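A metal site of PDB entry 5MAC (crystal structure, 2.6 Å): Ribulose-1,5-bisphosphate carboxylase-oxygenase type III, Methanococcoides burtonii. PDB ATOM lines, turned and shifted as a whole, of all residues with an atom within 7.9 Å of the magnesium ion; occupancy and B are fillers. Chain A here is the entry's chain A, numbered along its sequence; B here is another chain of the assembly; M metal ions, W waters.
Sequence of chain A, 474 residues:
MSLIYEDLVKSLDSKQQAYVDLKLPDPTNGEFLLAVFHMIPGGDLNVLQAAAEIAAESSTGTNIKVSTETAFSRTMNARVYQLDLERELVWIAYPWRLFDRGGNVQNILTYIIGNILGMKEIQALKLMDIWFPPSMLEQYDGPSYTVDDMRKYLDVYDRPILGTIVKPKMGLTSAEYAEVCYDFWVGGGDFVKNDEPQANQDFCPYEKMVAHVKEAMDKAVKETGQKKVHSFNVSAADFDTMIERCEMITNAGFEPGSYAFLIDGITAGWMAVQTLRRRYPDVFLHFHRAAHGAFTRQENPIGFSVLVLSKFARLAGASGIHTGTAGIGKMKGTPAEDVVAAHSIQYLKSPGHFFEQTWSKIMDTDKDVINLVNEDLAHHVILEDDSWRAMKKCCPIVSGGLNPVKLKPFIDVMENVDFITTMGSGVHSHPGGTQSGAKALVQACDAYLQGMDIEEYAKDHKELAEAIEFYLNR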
ATOM      1  N   GLU A 179      18.766 -26.252 -30.184  1.00  0.00           N
ATOM      2  CA  GLU A 179      19.994 -25.546 -29.815  1.00  0.00           C
ATOM      3  C   GLU A 179      20.104 -25.508 -28.327  1.00  0.00           C
ATOM      4  O   GLU A 179      21.204 -25.602 -27.792  1.00  0.00           O
ATOM      5  CB  GLU A 179      19.981 -24.100 -30.323  1.00  0.00           C
ATOM      6  CG  GLU A 179      21.284 -23.347 -30.078  1.00  0.00           C
ATOM      7  CD  GLU A 179      22.532 -23.938 -30.709  1.00  0.00           C
ATOM      8  OE1 GLU A 179      22.404 -24.670 -31.709  1.00  0.00           O
ATOM      9  OE2 GLU A 179      23.635 -23.638 -30.208  1.00  0.00           O
ATOM     10  N   VAL A 180      18.964 -25.306 -27.661  1.00  0.00           N
ATOM     11  CA  VAL A 180      18.921 -25.245 -26.203  1.00  0.00           C
ATOM     12  C   VAL A 180      19.324 -26.625 -25.647  1.00  0.00           C
ATOM     13  O   VAL A 180      20.076 -26.685 -24.683  1.00  0.00           O
ATOM     14  CB  VAL A 180      17.539 -24.744 -25.682  1.00  0.00           C
ATOM     15  CG1 VAL A 180      17.469 -24.798 -24.158  1.00  0.00           C
ATOM     16  CG2 VAL A 180      17.250 -23.324 -26.175  1.00  0.00           C
ATOM     17  N   TYR A 182      21.273 -29.108 -27.203  1.00  0.00           N
ATOM     18  CA  TYR A 182      22.712 -29.216 -27.445  1.00  0.00           C
ATOM     19  C   TYR A 182      23.558 -28.423 -26.418  1.00  0.00           C
ATOM     20  O   TYR A 182      24.504 -28.967 -25.873  1.00  0.00           O
ATOM     21  CB  TYR A 182      23.011 -28.725 -28.885  1.00  0.00           C
ATOM     22  CG  TYR A 182      24.485 -28.532 -29.143  1.00  0.00           C
ATOM     23  CD1 TYR A 182      25.293 -29.604 -29.505  1.00  0.00           C
ATOM     24  CD2 TYR A 182      25.089 -27.309 -28.879  1.00  0.00           C
ATOM     25  CE1 TYR A 182      26.665 -29.446 -29.644  1.00  0.00           C
ATOM     26  CE2 TYR A 182      26.456 -27.139 -29.023  1.00  0.00           C
ATOM     27  CZ  TYR A 182      27.246 -28.206 -29.416  1.00  0.00           C
ATOM     28  OH  TYR A 182      28.581 -28.010 -29.624  1.00  0.00           O
ATOM     29  N   ASP A 183      23.223 -27.146 -26.174  1.00  0.00           N
ATOM     30  CA  ASP A 183      23.990 -26.277 -25.263  1.00  0.00           C
ATOM     31  C   ASP A 183      24.041 -26.799 -23.835  1.00  0.00           C
ATOM     32  O   ASP A 183      25.058 -26.660 -23.156  1.00  0.00           O
ATOM     33  CB  ASP A 183      23.438 -24.838 -25.269  1.00  0.00           C
ATOM     34  CG  ASP A 183      23.645 -24.017 -26.539  1.00  0.00           C
ATOM     35  OD1 ASP A 183      24.648 -24.248 -27.239  1.00  0.00           O
ATOM     36  OD2 ASP A 183      22.838 -23.108 -26.799  1.00  0.00           O
ATOM     37  N   PHE A 184      22.940 -27.404 -23.358  1.00  0.00           N
ATOM     38  CA  PHE A 184      22.881 -27.949 -21.995  1.00  0.00           C
ATOM     39  C   PHE A 184      23.745 -29.190 -21.894  1.00  0.00           C
ATOM     40  O   PHE A 184      24.588 -29.287 -20.995  1.00  0.00           O
ATOM     41  CB  PHE A 184      21.441 -28.304 -21.585  1.00  0.00           C
ATOM     42  CG  PHE A 184      21.340 -28.832 -20.179  1.00  0.00           C
ATOM     43  CD1 PHE A 184      21.593 -28.006 -19.088  1.00  0.00           C
ATOM     44  CD2 PHE A 184      21.026 -30.166 -19.933  1.00  0.00           C
ATOM     45  CE1 PHE A 184      21.577 -28.512 -17.796  1.00  0.00           C
ATOM     46  CE2 PHE A 184      20.951 -30.646 -18.638  1.00  0.00           C
ATOM     47  CZ  PHE A 184      21.244 -29.820 -17.571  1.00  0.00           C
ATOM     48  N   VAL A 186      26.128 -30.308 -24.031  1.00  0.00           N
ATOM     49  CA  VAL A 186      27.549 -30.031 -24.290  1.00  0.00           C
ATOM     50  C   VAL A 186      28.249 -29.308 -23.081  1.00  0.00           C
ATOM     51  O   VAL A 186      29.464 -29.439 -22.905  1.00  0.00           O
ATOM     52  CB  VAL A 186      27.729 -29.301 -25.639  1.00  0.00           C
ATOM     53  CG1 VAL A 186      27.590 -27.797 -25.497  1.00  0.00           C
ATOM     54  CG2 VAL A 186      29.056 -29.684 -26.278  1.00  0.00           C
ATOM     55  N   THR A 434      22.884 -20.853 -21.583  1.00  0.00           N
ATOM     56  CA  THR A 434      22.678 -22.281 -21.297  1.00  0.00           C
ATOM     57  C   THR A 434      23.955 -23.087 -21.016  1.00  0.00           C
ATOM     58  O   THR A 434      23.969 -23.912 -20.090  1.00  0.00           O
ATOM     59  CB  THR A 434      21.884 -22.938 -22.447  1.00  0.00           C
ATOM     60  OG1 THR A 434      20.628 -22.302 -22.602  1.00  0.00           O
ATOM     61  CG2 THR A 434      21.667 -24.416 -22.254  1.00  0.00           C
ATOM     62  N   GLN A 435      25.002 -22.921 -21.830  1.00  0.00           N
ATOM     63  CA  GLN A 435      26.221 -23.709 -21.628  1.00  0.00           C
ATOM     64  C   GLN A 435      26.862 -23.359 -20.295  1.00  0.00           C
ATOM     65  O   GLN A 435      27.234 -24.269 -19.543  1.00  0.00           O
ATOM     66  CB  GLN A 435      27.229 -23.556 -22.784  1.00  0.00           C
ATOM     67  CG  GLN A 435      26.730 -23.977 -24.180  1.00  0.00           C
ATOM     68  CD  GLN A 435      27.847 -24.247 -25.138  1.00  0.00           C
ATOM     69  OE1 GLN A 435      28.989 -24.471 -24.748  1.00  0.00           O
ATOM     70  NE2 GLN A 435      27.522 -24.289 -26.433  1.00  0.00           N
ATOM     71  N   ILE B 362      18.074 -20.196 -35.893  1.00  0.00           N
ATOM     72  CA  ILE B 362      18.167 -19.815 -34.487  1.00  0.00           C
ATOM     73  C   ILE B 362      18.635 -18.349 -34.456  1.00  0.00           C
ATOM     74  O   ILE B 362      18.907 -17.778 -35.517  1.00  0.00           O
ATOM     75  CB  ILE B 362      19.076 -20.816 -33.681  1.00  0.00           C
ATOM     76  CG1 ILE B 362      20.564 -20.712 -34.097  1.00  0.00           C
ATOM     77  CG2 ILE B 362      18.568 -22.268 -33.861  1.00  0.00           C
ATOM     78  CD1 ILE B 362      21.566 -21.516 -33.237  1.00  0.00           C
ATOM     79  N   MET B 363      18.718 -17.723 -33.284  1.00  0.00           N
ATOM     80  CA  MET B 363      19.144 -16.303 -33.219  1.00  0.00           C
ATOM     81  C   MET B 363      20.634 -16.079 -33.563  1.00  0.00           C
ATOM     82  O   MET B 363      21.506 -16.849 -33.143  1.00  0.00           O
ATOM     83  CB  MET B 363      18.786 -15.653 -31.880  1.00  0.00           C
ATOM     84  CG  MET B 363      17.264 -15.478 -31.669  1.00  0.00           C
ATOM     85  SD  MET B 363      16.494 -14.176 -32.684  1.00  0.00           S
ATOM     86  CE  MET B 363      15.555 -13.237 -31.387  1.00  0.00           C
ATOM     87  N   THR B 365      22.724 -13.950 -32.463  1.00  0.00           N
ATOM     88  CA  THR B 365      23.538 -13.632 -31.307  1.00  0.00           C
ATOM     89  C   THR B 365      24.138 -14.907 -30.645  1.00  0.00           C
ATOM     90  O   THR B 365      25.037 -14.773 -29.798  1.00  0.00           O
ATOM     91  CB  THR B 365      22.733 -12.768 -30.321  1.00  0.00           C
ATOM     92  OG1 THR B 365      21.744 -13.581 -29.682  1.00  0.00           O
ATOM     93  CG2 THR B 365      22.047 -11.557 -31.013  1.00  0.00           C
ATOM     94  N   ASP B 366      23.654 -16.118 -31.006  1.00  0.00           N
ATOM     95  CA  ASP B 366      24.203 -17.346 -30.421  1.00  0.00           C
ATOM     96  C   ASP B 366      25.663 -17.426 -30.863  1.00  0.00           C
ATOM     97  O   ASP B 366      25.941 -17.261 -32.053  1.00  0.00           O
ATOM     98  CB  ASP B 366      23.435 -18.603 -30.889  1.00  0.00           C
ATOM     99  CG  ASP B 366      23.588 -19.814 -29.972  1.00  0.00           C
ATOM    100  OD1 ASP B 366      24.732 -20.253 -29.760  1.00  0.00           O
ATOM    101  OD2 ASP B 366      22.559 -20.338 -29.489  1.00  0.00           O
ATOM    102  N   LYS B 367      26.587 -17.612 -29.921  1.00  0.00           N
ATOM    103  CA  LYS B 367      28.006 -17.701 -30.221  1.00  0.00           C
ATOM    104  C   LYS B 367      28.280 -18.766 -31.287  1.00  0.00           C
ATOM    105  O   LYS B 367      29.206 -18.614 -32.094  1.00  0.00           O
ATOM    106  CB  LYS B 367      28.805 -18.004 -28.932  1.00  0.00           C
ATOM    107  CG  LYS B 367      30.335 -18.164 -29.113  1.00  0.00           C
ATOM    108  CD  LYS B 367      31.035 -17.003 -29.849  1.00  0.00           C
ATOM    109  CE  LYS B 367      32.516 -17.261 -30.001  1.00  0.00           C
ATOM    110  NZ  LYS B 367      33.105 -16.480 -31.107  1.00  0.00           N
ATOM    111  N   ASP B 368      27.448 -19.827 -31.318  1.00  0.00           N
ATOM    112  CA  ASP B 368      27.560 -20.908 -32.299  1.00  0.00           C
ATOM    113  C   ASP B 368      27.237 -20.411 -33.734  1.00  0.00           C
ATOM    114  O   ASP B 368      27.803 -20.952 -34.685  1.00  0.00           O
ATOM    115  CB  ASP B 368      26.661 -22.089 -31.884  1.00  0.00           C
ATOM    116  CG  ASP B 368      27.050 -22.738 -30.550  1.00  0.00           C
ATOM    117  OD1 ASP B 368      28.169 -23.315 -30.475  1.00  0.00           O
ATOM    118  OD2 ASP B 368      26.239 -22.687 -29.597  1.00  0.00           O
ATOM    119  N   VAL B 369      26.353 -19.401 -33.885  1.00  0.00           N
ATOM    120  CA  VAL B 369      26.023 -18.776 -35.176  1.00  0.00           C
ATOM    121  C   VAL B 369      27.143 -17.819 -35.564  1.00  0.00           C
ATOM    122  O   VAL B 369      27.525 -17.776 -36.741  1.00  0.00           O
ATOM    123  CB  VAL B 369      24.634 -18.096 -35.204  1.00  0.00           C
ATOM    124  CG1 VAL B 369      24.433 -17.257 -36.479  1.00  0.00           C
ATOM    125  CG2 VAL B 369      23.528 -19.132 -35.093  1.00  0.00           C
ATOM    126  N   TRP B 388      20.419 -28.175 -38.119  1.00  0.00           N
ATOM    127  CA  TRP B 388      19.287 -27.480 -37.471  1.00  0.00           C
ATOM    128  C   TRP B 388      19.496 -25.945 -37.365  1.00  0.00           C
ATOM    129  O   TRP B 388      18.529 -25.193 -37.297  1.00  0.00           O
ATOM    130  CB  TRP B 388      19.009 -28.060 -36.032  1.00  0.00           C
ATOM    131  CG  TRP B 388      19.918 -27.567 -34.923  1.00  0.00           C
ATOM    132  CD1 TRP B 388      19.755 -26.435 -34.173  1.00  0.00           C
ATOM    133  CD2 TRP B 388      21.067 -28.236 -34.390  1.00  0.00           C
ATOM    134  NE1 TRP B 388      20.772 -26.320 -33.248  1.00  0.00           N
ATOM    135  CE2 TRP B 388      21.581 -27.422 -33.356  1.00  0.00           C
ATOM    136  CE3 TRP B 388      21.712 -29.456 -34.667  1.00  0.00           C
ATOM    137  CZ2 TRP B 388      22.728 -27.775 -32.617  1.00  0.00           C
ATOM    138  CZ3 TRP B 388      22.837 -29.809 -33.928  1.00  0.00           C
ATOM    139  CH2 TRP B 388      23.336 -28.965 -32.945  1.00  0.00           C
ATOM    140  N   ARG B 389      20.738 -25.518 -37.285  1.00  0.00           N
ATOM    141  CA  ARG B 389      21.101 -24.126 -37.042  1.00  0.00           C
ATOM    142  C   ARG B 389      20.859 -23.187 -38.164  1.00  0.00           C
ATOM    143  O   ARG B 389      20.651 -22.007 -37.905  1.00  0.00           O
ATOM    144  CB  ARG B 389      22.593 -24.068 -36.651  1.00  0.00           C
ATOM    145  CG  ARG B 389      22.905 -24.796 -35.355  1.00  0.00           C
ATOM    146  CD  ARG B 389      24.325 -24.557 -34.949  1.00  0.00           C
ATOM    147  NE  ARG B 389      24.567 -24.942 -33.556  1.00  0.00           N
ATOM    148  CZ  ARG B 389      25.745 -25.273 -33.042  1.00  0.00           C
ATOM    149  NH1 ARG B 389      26.841 -25.296 -33.806  1.00  0.00           N
ATOM    150  NH2 ARG B 389      25.853 -25.568 -31.757  1.00  0.00           N
HETATM  151 MG    MG M   1      24.628 -22.201 -28.608  1.00  0.00          MG
HETATM  152  O   HOH W   1      26.568 -20.632 -27.185  1.00  0.00           O
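OD2 of Asp 368 of chain B is bound to the magnesium ion, 2.0 Å away. The side-chain carboxylate (OD1) of Asp 366 of chain B binds the magnesium ion (2.3 Å). The magnesium ion is bound by the side-chain carboxylate (OE2) of Glu 179, at 2.4 Å. The magnesium ion is bound by OD1 of Asp 183, 2.5 Å away. The magnesium ion has four donor atoms within binding distance. Slightly farther from the magnesium ion lies the side-chain carboxylate (OD2) of Asp 183 (2.7 Å).
Four residues have an atom within 4 Å of the magnesium ion: Glu 179, Asp 183, Asp 366 of chain B and Asp 368 of chain B. The nearest printed residue that does not touch the magnesium ion is Gln 435 (4.2 Å).
The side-chain carboxylate of Asp 368 of chain B lies within salt-bridge range of the guanidinium group of Arg 389 of chain B. The side-chain carboxylate (OD1) of Asp 183 lies close to the side-chain amide nitrogen (NE2) of Gln 435 (3.0 Å). NE1 of Trp 388 of chain B lies within hydrogen-bond range of OE1 of Glu 179, 2.8 Å away. The guanidinium group (NE) of Arg 389 of chain B is in salt-bridge range of the side-chain carboxylate (OE1) of Glu 179, 2.9 Å away.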
